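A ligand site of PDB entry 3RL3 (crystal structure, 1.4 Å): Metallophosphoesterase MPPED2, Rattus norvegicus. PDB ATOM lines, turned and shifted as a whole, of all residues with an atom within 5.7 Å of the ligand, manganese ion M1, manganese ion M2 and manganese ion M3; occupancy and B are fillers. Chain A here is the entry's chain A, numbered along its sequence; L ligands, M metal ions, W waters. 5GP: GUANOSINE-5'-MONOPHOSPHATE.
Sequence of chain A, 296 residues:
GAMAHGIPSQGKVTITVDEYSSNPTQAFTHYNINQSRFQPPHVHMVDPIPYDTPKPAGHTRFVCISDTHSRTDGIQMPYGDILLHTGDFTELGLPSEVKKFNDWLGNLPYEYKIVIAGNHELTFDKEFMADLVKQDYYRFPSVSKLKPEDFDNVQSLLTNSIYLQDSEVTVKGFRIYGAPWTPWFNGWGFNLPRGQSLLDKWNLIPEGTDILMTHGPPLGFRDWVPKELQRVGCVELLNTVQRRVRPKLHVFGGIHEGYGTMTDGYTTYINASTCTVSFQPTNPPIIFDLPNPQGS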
ATOM      1  N   ASP A  67     -18.847  12.278 -10.497  1.00  0.00           N
ATOM      2  CA  ASP A  67     -18.673  13.742 -10.679  1.00  0.00           C
ATOM      3  C   ASP A  67     -17.366  14.203 -10.043  1.00  0.00           C
ATOM      4  O   ASP A  67     -17.324  15.177  -9.293  1.00  0.00           O
ATOM      5  CB  ASP A  67     -19.886  14.477 -10.091  1.00  0.00           C
ATOM      6  CG  ASP A  67     -21.146  14.170 -10.885  1.00  0.00           C
ATOM      7  OD1 ASP A  67     -21.388  14.878 -11.894  1.00  0.00           O
ATOM      8  OD2 ASP A  67     -21.870  13.216 -10.496  1.00  0.00           O
ATOM      9  N   HIS A  69     -14.771  15.046 -12.067  1.00  0.00           N
ATOM     10  CA  HIS A  69     -14.428  16.193 -12.917  1.00  0.00           C
ATOM     11  C   HIS A  69     -12.928  16.428 -12.994  1.00  0.00           C
ATOM     12  O   HIS A  69     -12.473  17.572 -12.999  1.00  0.00           O
ATOM     13  CB  HIS A  69     -15.191  17.436 -12.449  1.00  0.00           C
ATOM     14  CG  HIS A  69     -16.650  17.405 -12.789  1.00  0.00           C
ATOM     15  ND1 HIS A  69     -17.116  17.691 -14.050  1.00  0.00           N
ATOM     16  CD2 HIS A  69     -17.734  17.081 -12.046  1.00  0.00           C
ATOM     17  CE1 HIS A  69     -18.433  17.567 -14.071  1.00  0.00           C
ATOM     18  NE2 HIS A  69     -18.842  17.194 -12.864  1.00  0.00           N
ATOM     19  N   GLY A  87     -20.069   8.722 -13.361  1.00  0.00           N
ATOM     20  CA  GLY A  87     -19.926   9.620 -14.538  1.00  0.00           C
ATOM     21  C   GLY A  87     -19.430  11.018 -14.228  1.00  0.00           C
ATOM     22  O   GLY A  87     -19.259  11.400 -13.051  1.00  0.00           O
ATOM     23  N   ASP A  88     -19.210  11.814 -15.273  1.00  0.00           N
ATOM     24  CA  ASP A  88     -18.524  13.090 -15.143  1.00  0.00           C
ATOM     25  C   ASP A  88     -17.171  12.867 -14.469  1.00  0.00           C
ATOM     26  O   ASP A  88     -16.815  13.535 -13.474  1.00  0.00           O
ATOM     27  CB  ASP A  88     -19.351  14.145 -14.375  1.00  0.00           C
ATOM     28  CG  ASP A  88     -20.434  14.790 -15.239  1.00  0.00           C
ATOM     29  OD1 ASP A  88     -20.562  14.461 -16.442  1.00  0.00           O
ATOM     30  OD2 ASP A  88     -21.177  15.623 -14.686  1.00  0.00           O
ATOM     31  N   GLY A 118     -20.963  10.334 -17.928  1.00  0.00           N
ATOM     32  CA  GLY A 118     -21.964  11.365 -17.727  1.00  0.00           C
ATOM     33  C   GLY A 118     -21.971  12.364 -18.874  1.00  0.00           C
ATOM     34  O   GLY A 118     -21.355  12.129 -19.934  1.00  0.00           O
ATOM     35  N   ASN A 119     -22.633  13.490 -18.649  1.00  0.00           N
ATOM     36  CA  ASN A 119     -22.793  14.492 -19.735  1.00  0.00           C
ATOM     37  C   ASN A 119     -21.502  15.186 -20.134  1.00  0.00           C
ATOM     38  O   ASN A 119     -21.406  15.716 -21.246  1.00  0.00           O
ATOM     39  CB  ASN A 119     -23.889  15.502 -19.413  1.00  0.00           C
ATOM     40  CG  ASN A 119     -23.662  16.180 -18.131  1.00  0.00           C
ATOM     41  OD1 ASN A 119     -23.420  15.536 -17.116  1.00  0.00           O
ATOM     42  ND2 ASN A 119     -23.790  17.492 -18.121  1.00  0.00           N
ATOM     43  N   HIS A 120     -20.513  15.177 -19.248  1.00  0.00           N
ATOM     44  CA  HIS A 120     -19.245  15.827 -19.608  1.00  0.00           C
ATOM     45  C   HIS A 120     -18.353  14.958 -20.501  1.00  0.00           C
ATOM     46  O   HIS A 120     -17.381  15.471 -21.073  1.00  0.00           O
ATOM     47  CB  HIS A 120     -18.478  16.294 -18.373  1.00  0.00           C
ATOM     48  CG  HIS A 120     -19.035  17.550 -17.768  1.00  0.00           C
ATOM     49  ND1 HIS A 120     -18.411  18.771 -17.882  1.00  0.00           N
ATOM     50  CD2 HIS A 120     -20.197  17.786 -17.107  1.00  0.00           C
ATOM     51  CE1 HIS A 120     -19.131  19.695 -17.273  1.00  0.00           C
ATOM     52  NE2 HIS A 120     -20.241  19.127 -16.819  1.00  0.00           N
ATOM     53  N   PRO A 183     -32.050  13.628 -18.454  1.00  0.00           N
ATOM     54  CA  PRO A 183     -32.981  14.551 -19.119  1.00  0.00           C
ATOM     55  C   PRO A 183     -32.264  15.775 -19.691  1.00  0.00           C
ATOM     56  O   PRO A 183     -31.350  16.315 -19.069  1.00  0.00           O
ATOM     57  CB  PRO A 183     -33.968  14.951 -18.025  1.00  0.00           C
ATOM     58  CG  PRO A 183     -33.750  14.023 -16.857  1.00  0.00           C
ATOM     59  CD  PRO A 183     -32.389  13.385 -17.032  1.00  0.00           C
ATOM     60  N   TRP A 184     -32.680  16.183 -20.889  1.00  0.00           N
ATOM     61  CA  TRP A 184     -32.033  17.263 -21.617  1.00  0.00           C
ATOM     62  C   TRP A 184     -31.864  18.485 -20.726  1.00  0.00           C
ATOM     63  O   TRP A 184     -32.804  18.931 -20.081  1.00  0.00           O
ATOM     64  CB  TRP A 184     -32.873  17.633 -22.850  1.00  0.00           C
ATOM     65  CG  TRP A 184     -32.049  18.357 -23.920  1.00  0.00           C
ATOM     66  CD1 TRP A 184     -31.424  17.779 -24.986  1.00  0.00           C
ATOM     67  CD2 TRP A 184     -31.798  19.755 -24.006  1.00  0.00           C
ATOM     68  NE1 TRP A 184     -30.784  18.756 -25.729  1.00  0.00           N
ATOM     69  CE2 TRP A 184     -30.991  19.965 -25.145  1.00  0.00           C
ATOM     70  CE3 TRP A 184     -32.178  20.863 -23.234  1.00  0.00           C
ATOM     71  CZ2 TRP A 184     -30.566  21.244 -25.534  1.00  0.00           C
ATOM     72  CZ3 TRP A 184     -31.745  22.136 -23.620  1.00  0.00           C
ATOM     73  CH2 TRP A 184     -30.941  22.300 -24.752  1.00  0.00           C
ATOM     74  N   PHE A 185     -30.644  18.995 -20.687  1.00  0.00           N
ATOM     75  CA  PHE A 185     -30.335  20.146 -19.881  1.00  0.00           C
ATOM     76  C   PHE A 185     -29.648  21.195 -20.752  1.00  0.00           C
ATOM     77  O   PHE A 185     -30.240  22.243 -21.011  1.00  0.00           O
ATOM     78  CB  PHE A 185     -29.493  19.724 -18.676  1.00  0.00           C
ATOM     79  CG  PHE A 185     -29.104  20.854 -17.782  1.00  0.00           C
ATOM     80  CD1 PHE A 185     -30.059  21.750 -17.303  1.00  0.00           C
ATOM     81  CD2 PHE A 185     -27.785  20.997 -17.373  1.00  0.00           C
ATOM     82  CE1 PHE A 185     -29.679  22.806 -16.468  1.00  0.00           C
ATOM     83  CE2 PHE A 185     -27.397  22.034 -16.528  1.00  0.00           C
ATOM     84  CZ  PHE A 185     -28.359  22.943 -16.080  1.00  0.00           C
ATOM     85  N   ASN A 186     -28.461  20.897 -21.265  1.00  0.00           N
ATOM     86  CA  ASN A 186     -27.687  21.861 -22.081  1.00  0.00           C
ATOM     87  C   ASN A 186     -27.282  21.284 -23.427  1.00  0.00           C
ATOM     88  O   ASN A 186     -26.515  21.912 -24.174  1.00  0.00           O
ATOM     89  CB  ASN A 186     -26.390  22.300 -21.389  1.00  0.00           C
ATOM     90  CG  ASN A 186     -26.619  22.964 -20.048  1.00  0.00           C
ATOM     91  OD1 ASN A 186     -27.479  23.831 -19.894  1.00  0.00           O
ATOM     92  ND2 ASN A 186     -25.801  22.582 -19.063  1.00  0.00           N
ATOM     93  N   ARG A 194     -37.232  14.342 -21.883  1.00  0.00           N
ATOM     94  CA  ARG A 194     -38.071  13.574 -20.993  1.00  0.00           C
ATOM     95  C   ARG A 194     -39.143  12.801 -21.743  1.00  0.00           C
ATOM     96  O   ARG A 194     -39.602  13.201 -22.820  1.00  0.00           O
ATOM     97  CB  ARG A 194     -38.699  14.508 -19.956  1.00  0.00           C
ATOM     98  CG  ARG A 194     -37.682  15.063 -18.976  1.00  0.00           C
ATOM     99  CD  ARG A 194     -38.307  16.002 -17.930  1.00  0.00           C
ATOM    100  NE  ARG A 194     -37.260  16.691 -17.164  1.00  0.00           N
ATOM    101  CZ  ARG A 194     -36.697  16.199 -16.071  1.00  0.00           C
ATOM    102  NH1 ARG A 194     -37.059  15.018 -15.594  1.00  0.00           N
ATOM    103  NH2 ARG A 194     -35.745  16.905 -15.449  1.00  0.00           N
ATOM    104  N   HIS A 215     -26.245   8.286 -14.506  1.00  0.00           N
ATOM    105  CA  HIS A 215     -25.500   9.491 -14.183  1.00  0.00           C
ATOM    106  C   HIS A 215     -26.313  10.403 -13.284  1.00  0.00           C
ATOM    107  O   HIS A 215     -25.779  11.014 -12.371  1.00  0.00           O
ATOM    108  CB  HIS A 215     -25.005  10.227 -15.416  1.00  0.00           C
ATOM    109  CG  HIS A 215     -24.277  11.497 -15.069  1.00  0.00           C
ATOM    110  ND1 HIS A 215     -23.195  11.508 -14.202  1.00  0.00           N
ATOM    111  CD2 HIS A 215     -24.479  12.786 -15.447  1.00  0.00           C
ATOM    112  CE1 HIS A 215     -22.778  12.753 -14.050  1.00  0.00           C
ATOM    113  NE2 HIS A 215     -23.534  13.555 -14.790  1.00  0.00           N
ATOM    114  N   VAL A 225     -32.665  20.847  -6.878  1.00  0.00           N
ATOM    115  CA  VAL A 225     -31.721  21.867  -7.348  1.00  0.00           C
ATOM    116  C   VAL A 225     -32.103  23.191  -6.661  1.00  0.00           C
ATOM    117  O   VAL A 225     -33.067  23.837  -7.074  1.00  0.00           O
ATOM    118  CB  VAL A 225     -31.729  21.988  -8.899  1.00  0.00           C
ATOM    119  CG1 VAL A 225     -30.748  23.045  -9.382  1.00  0.00           C
ATOM    120  CG2 VAL A 225     -31.397  20.639  -9.541  1.00  0.00           C
ATOM    121  N   LYS A 227     -30.987  26.242  -6.582  1.00  0.00           N
ATOM    122  CA  LYS A 227     -30.978  27.490  -7.340  1.00  0.00           C
ATOM    123  C   LYS A 227     -32.249  27.654  -8.152  1.00  0.00           C
ATOM    124  O   LYS A 227     -32.704  28.775  -8.368  1.00  0.00           O
ATOM    125  CB  LYS A 227     -29.726  27.637  -8.218  1.00  0.00           C
ATOM    126  CG  LYS A 227     -29.616  26.686  -9.374  1.00  0.00           C
ATOM    127  CD  LYS A 227     -28.161  26.506  -9.780  1.00  0.00           C
ATOM    128  CE  LYS A 227     -27.952  25.152 -10.441  1.00  0.00           C
ATOM    129  NZ  LYS A 227     -26.518  24.855 -10.660  1.00  0.00           N
ATOM    130  N   GLU A 228     -32.820  26.526  -8.598  1.00  0.00           N
ATOM    131  CA  GLU A 228     -34.020  26.550  -9.425  1.00  0.00           C
ATOM    132  C   GLU A 228     -35.296  26.303  -8.633  1.00  0.00           C
ATOM    133  O   GLU A 228     -36.398  26.482  -9.172  1.00  0.00           O
ATOM    134  CB  GLU A 228     -33.932  25.509 -10.549  1.00  0.00           C
ATOM    135  CG  GLU A 228     -32.918  25.849 -11.619  1.00  0.00           C
ATOM    136  CD  GLU A 228     -33.312  27.086 -12.400  1.00  0.00           C
ATOM    137  OE1 GLU A 228     -34.094  26.977 -13.374  1.00  0.00           O
ATOM    138  OE2 GLU A 228     -32.844  28.184 -12.026  1.00  0.00           O
ATOM    139  N   GLN A 230     -36.456  23.439  -7.833  1.00  0.00           N
ATOM    140  CA  GLN A 230     -37.106  22.427  -8.646  1.00  0.00           C
ATOM    141  C   GLN A 230     -36.501  21.059  -8.385  1.00  0.00           C
ATOM    142  O   GLN A 230     -35.290  20.930  -8.118  1.00  0.00           O
ATOM    143  CB  GLN A 230     -36.967  22.748 -10.131  1.00  0.00           C
ATOM    144  CG  GLN A 230     -37.909  23.851 -10.627  1.00  0.00           C
ATOM    145  CD  GLN A 230     -38.078  23.855 -12.132  1.00  0.00           C
ATOM    146  OE1 GLN A 230     -37.198  23.404 -12.866  1.00  0.00           O
ATOM    147  NE2 GLN A 230     -39.213  24.373 -12.590  1.00  0.00           N
ATOM    148  N   VAL A 232     -35.513  17.645 -10.353  1.00  0.00           N
ATOM    149  CA  VAL A 232     -35.138  17.431 -11.750  1.00  0.00           C
ATOM    150  C   VAL A 232     -34.915  15.957 -12.120  1.00  0.00           C
ATOM    151  O   VAL A 232     -34.515  15.657 -13.252  1.00  0.00           O
ATOM    152  CB  VAL A 232     -33.882  18.251 -12.161  1.00  0.00           C
ATOM    153  CG1 VAL A 232     -34.111  19.763 -11.941  1.00  0.00           C
ATOM    154  CG2 VAL A 232     -32.646  17.789 -11.398  1.00  0.00           C
ATOM    155  N   GLY A 254     -24.788  13.474 -10.740  1.00  0.00           N
ATOM    156  CA  GLY A 254     -25.497  14.384 -11.646  1.00  0.00           C
ATOM    157  C   GLY A 254     -25.814  15.708 -10.991  1.00  0.00           C
ATOM    158  O   GLY A 254     -25.310  16.759 -11.413  1.00  0.00           O
ATOM    159  N   ILE A 255     -26.662  15.642  -9.976  1.00  0.00           N
ATOM    160  CA  ILE A 255     -27.003  16.834  -9.172  1.00  0.00           C
ATOM    161  C   ILE A 255     -26.057  16.872  -7.990  1.00  0.00           C
ATOM    162  O   ILE A 255     -26.259  16.156  -6.993  1.00  0.00           O
ATOM    163  CB  ILE A 255     -28.484  16.791  -8.755  1.00  0.00           C
ATOM    164  CG1 ILE A 255     -29.377  16.666 -10.009  1.00  0.00           C
ATOM    165  CG2 ILE A 255     -28.871  18.033  -7.921  1.00  0.00           C
ATOM    166  CD1 ILE A 255     -29.129  17.750 -11.110  1.00  0.00           C
ATOM    167  N   HIS A 256     -24.993  17.661  -8.116  1.00  0.00           N
ATOM    168  CA  HIS A 256     -23.918  17.636  -7.096  1.00  0.00           C
ATOM    169  C   HIS A 256     -24.471  17.967  -5.720  1.00  0.00           C
ATOM    170  O   HIS A 256     -24.049  17.369  -4.708  1.00  0.00           O
ATOM    171  CB  HIS A 256     -22.797  18.619  -7.436  1.00  0.00           C
ATOM    172  CG  HIS A 256     -22.084  18.342  -8.725  1.00  0.00           C
ATOM    173  ND1 HIS A 256     -20.995  19.085  -9.128  1.00  0.00           N
ATOM    174  CD2 HIS A 256     -22.285  17.421  -9.711  1.00  0.00           C
ATOM    175  CE1 HIS A 256     -20.566  18.666 -10.302  1.00  0.00           C
ATOM    176  NE2 HIS A 256     -21.330  17.650 -10.685  1.00  0.00           N
ATOM    177  N   GLU A 257     -25.402  18.912  -5.697  1.00  0.00           N
ATOM    178  CA  GLU A 257     -26.056  19.381  -4.446  1.00  0.00           C
ATOM    179  C   GLU A 257     -26.759  18.282  -3.675  1.00  0.00           C
ATOM    180  O   GLU A 257     -27.045  18.426  -2.472  1.00  0.00           O
ATOM    181  CB  GLU A 257     -27.094  20.485  -4.748  1.00  0.00           C
ATOM    182  CG  GLU A 257     -26.602  21.692  -5.499  1.00  0.00           C
ATOM    183  CD  GLU A 257     -26.782  21.535  -6.990  1.00  0.00           C
ATOM    184  OE1 GLU A 257     -26.144  20.642  -7.556  1.00  0.00           O
ATOM    185  OE2 GLU A 257     -27.511  22.304  -7.642  1.00  0.00           O
ATOM    186  N   VAL A 277     -21.433  21.815  -5.855  1.00  0.00           N
ATOM    187  CA  VAL A 277     -21.965  22.588  -6.988  1.00  0.00           C
ATOM    188  C   VAL A 277     -20.930  23.616  -7.507  1.00  0.00           C
ATOM    189  O   VAL A 277     -21.020  24.067  -8.653  1.00  0.00           O
ATOM    190  CB  VAL A 277     -23.332  23.265  -6.625  1.00  0.00           C
ATOM    191  CG1 VAL A 277     -23.116  24.382  -5.602  1.00  0.00           C
ATOM    192  CG2 VAL A 277     -24.044  23.779  -7.898  1.00  0.00           C
ATOM    193  N   PHE A 279     -17.772  22.759  -7.722  1.00  0.00           N
ATOM    194  CA  PHE A 279     -16.754  21.899  -8.309  1.00  0.00           C
ATOM    195  C   PHE A 279     -15.548  21.647  -7.403  1.00  0.00           C
ATOM    196  O   PHE A 279     -14.432  21.420  -7.879  1.00  0.00           O
ATOM    197  CB  PHE A 279     -16.359  22.391  -9.719  1.00  0.00           C
ATOM    198  CG  PHE A 279     -17.391  22.052 -10.780  1.00  0.00           C
ATOM    199  CD1 PHE A 279     -18.590  22.746 -10.848  1.00  0.00           C
ATOM    200  CD2 PHE A 279     -17.159  21.024 -11.697  1.00  0.00           C
ATOM    201  CE1 PHE A 279     -19.551  22.417 -11.839  1.00  0.00           C
ATOM    202  CE2 PHE A 279     -18.101  20.704 -12.675  1.00  0.00           C
ATOM    203  CZ  PHE A 279     -19.300  21.398 -12.743  1.00  0.00           C
HETATM  204  P   5GP L   1     -22.732  18.991 -14.573  1.00  0.00           P
HETATM  205  O1P 5GP L   1     -23.421  17.872 -15.300  1.00  0.00           O
HETATM  206  O2P 5GP L   1     -21.400  18.543 -13.812  1.00  0.00           O
HETATM  207  O3P 5GP L   1     -22.375  20.133 -15.586  1.00  0.00           O
HETATM  208  O5' 5GP L   1     -23.752  19.597 -13.483  1.00  0.00           O
HETATM  209  C5' 5GP L   1     -23.293  20.516 -12.493  1.00  0.00           C
HETATM  210  C4' 5GP L   1     -24.531  21.165 -11.801  1.00  0.00           C
HETATM  211  O4' 5GP L   1     -25.430  21.672 -12.832  1.00  0.00           O
HETATM  212  C3' 5GP L   1     -25.451  20.227 -11.018  1.00  0.00           C
HETATM  213  O3' 5GP L   1     -24.915  20.009  -9.739  1.00  0.00           O
HETATM  214  C2' 5GP L   1     -26.734  21.056 -10.950  1.00  0.00           C
HETATM  215  O2' 5GP L   1     -26.591  22.210 -10.079  1.00  0.00           O
HETATM  216  C1' 5GP L   1     -26.791  21.558 -12.381  1.00  0.00           C
HETATM  217  N9  5GP L   1     -27.572  20.588 -13.180  1.00  0.00           N
HETATM  218  C8  5GP L   1     -27.164  19.434 -13.716  1.00  0.00           C
HETATM  219  N7  5GP L   1     -28.188  18.858 -14.353  1.00  0.00           N
HETATM  220  C5  5GP L   1     -29.251  19.646 -14.217  1.00  0.00           C
HETATM  221  C6  5GP L   1     -30.580  19.580 -14.638  1.00  0.00           C
HETATM  222  O6  5GP L   1     -30.982  18.641 -15.319  1.00  0.00           O
HETATM  223  N1  5GP L   1     -31.450  20.614 -14.306  1.00  0.00           N
HETATM  224  C2  5GP L   1     -30.970  21.696 -13.548  1.00  0.00           C
HETATM  225  N2  5GP L   1     -31.780  22.701 -13.229  1.00  0.00           N
HETATM  226  N3  5GP L   1     -29.694  21.727 -13.148  1.00  0.00           N
HETATM  227  C4  5GP L   1     -28.852  20.742 -13.466  1.00  0.00           C
HETATM  228 MN    MN M   1     -21.035  16.766 -12.752  1.00  0.00          MN
HETATM  229 MN    MN M   2     -23.417  15.792 -15.081  1.00  0.00          MN
HETATM  230 MN    MN M   3     -23.062  21.990 -16.281  1.00  0.00          MN
HETATM  231  O   HOH W   1     -33.394  18.627 -17.166  1.00  0.00           O
HETATM  232  O   HOH W   2     -27.773  15.676 -13.704  1.00  0.00           O
HETATM  233  O   HOH W   3     -29.827  16.558 -16.860  1.00  0.00           O
HETATM  234  O   HOH W   4     -25.937  24.764 -14.107  1.00  0.00           O
HETATM  235  O   HOH W   5     -23.582  20.710 -18.235  1.00  0.00           O
HETATM  236  O   HOH W   6     -23.302  16.216 -12.960  1.00  0.00           O
HETATM  237  O   HOH W   7     -25.531  15.813 -15.278  1.00  0.00           O
HETATM  238  O   HOH W   8     -21.799  22.818 -15.443  1.00  0.00           O
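Manganese ion M2 is bound by the side-chain amide oxygen (OD1) of Asn 119 (2.1 Å), an oxygen (O1P) of the ligand (2.1 Å), water W7 (2.1 Å), water W6 (2.2 Å), a ring nitrogen (NE2) of His 215 (2.3 Å) and the side-chain carboxylate (OD2) of Asp 88 (2.3 Å).
O2' of the ligand lies within hydrogen-bond range of NZ of Lys 227 (2.7 Å).
O3' of the ligand lies within hydrogen-bond range of N of His 256, at 2.9 Å.
A ring nitrogen (NE2) of His 120 sits close to an oxygen (O3P) of the ligand, at 2.7 Å.
The side-chain carboxylate (OE1) of Glu 257 sits at hydrogen-bond distance from an oxygen (O3') of the ligand, at 2.6 Å.
Manganese ion M1 is bound by O2P of the ligand (2.1 Å), OD1 of Asp 67 (2.1 Å), NE2 of His 69 (2.2 Å), OD2 of Asp 88 (2.3 Å), NE2 of His 256 (2.3 Å) and water W6 (2.3 Å).
Manganese ion M1 has six donor atoms within binding distance.
Merely in contact with manganese ion M3: Asn 186 (3.9 Å).
Water W6 lies within hydrogen-bond range of O of Gly 254 (2.6 Å) and O5' of the ligand (3.5 Å).
Water W5 bridges ND2 of Asn 186 (3.0 Å) and ND2 of Asn 119 (3.2 Å).
Water W3 bridges O of Pro 183 and O6 of the ligand.
Water W1 lies within hydrogen-bond range of O of Trp 184 (3.0 Å), O6 of the ligand (3.0 Å) and NH2 of Arg 194 (3.4 Å).
Water W4 bridges an oxygen (O4') of the ligand (3.4 Å) and the side-chain amino group (NZ) of Lys 227 (3.5 Å).
Manganese ion M3 is bound by water W8.
Manganese ion M3 is bound by O3P of the ligand (2.1 Å).
Manganese ion M3 is bound by water W5, at 2.4 Å.
Manganese ion M3 has three donor atoms within binding distance.
CE1 of Phe 185 touches C2 of the ligand (3.4 Å).
Val 225 touches the ligand (CG1 to N2, 3.998 Å).
CG of Glu 228 touches N2 of the ligand, at 3.7 Å.
Val 232 touches the ligand (CG1 to N1, 3.7 Å).
O of Gly 254 touches C3' of the ligand, 3.5 Å away.
Ile 255 touches the ligand (CD1 to N7, 3.6 Å).
Val 277 touches the ligand (CG2 to O2', 3.7 Å).
Phe 279 touches the ligand (CZ to O2P, 3.7 Å).
Hydrophobic or aromatic side chains within 4 Å of the ligand: His 69, His 120, Phe 185, Val 225, Val 232, Ile 255, His 256, Val 277 and Phe 279.
The guanidinium group (NH2) of Arg 194 lies within hydrogen-bond range of the backbone carbonyl oxygen (O) of Val 232, at 2.8 Å.
The backbone NH of Asp 67 sits at hydrogen-bond distance from the backbone carbonyl oxygen of Gly 87, at 2.7 Å.
The backbone carbonyl oxygen of His 215 is in hydrogen-bond range of the backbone NH of Gly 254.
OD1 of Asp 88 lies within hydrogen-bond range of N of His 120.
The backbone NH (N) of Val 225 lies within hydrogen-bond range of the backbone carbonyl oxygen (O) of Gln 230.
The backbone NH of Gly 254 is in hydrogen-bond range of the side-chain carboxylate of Asp 67 (2.9 Å).
The nearest printed residue that does not touch manganese ion M2 is Gly 254 (4.2 Å).
Of the 24 residues printed, 4 come within 4 Å of manganese ion M1.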
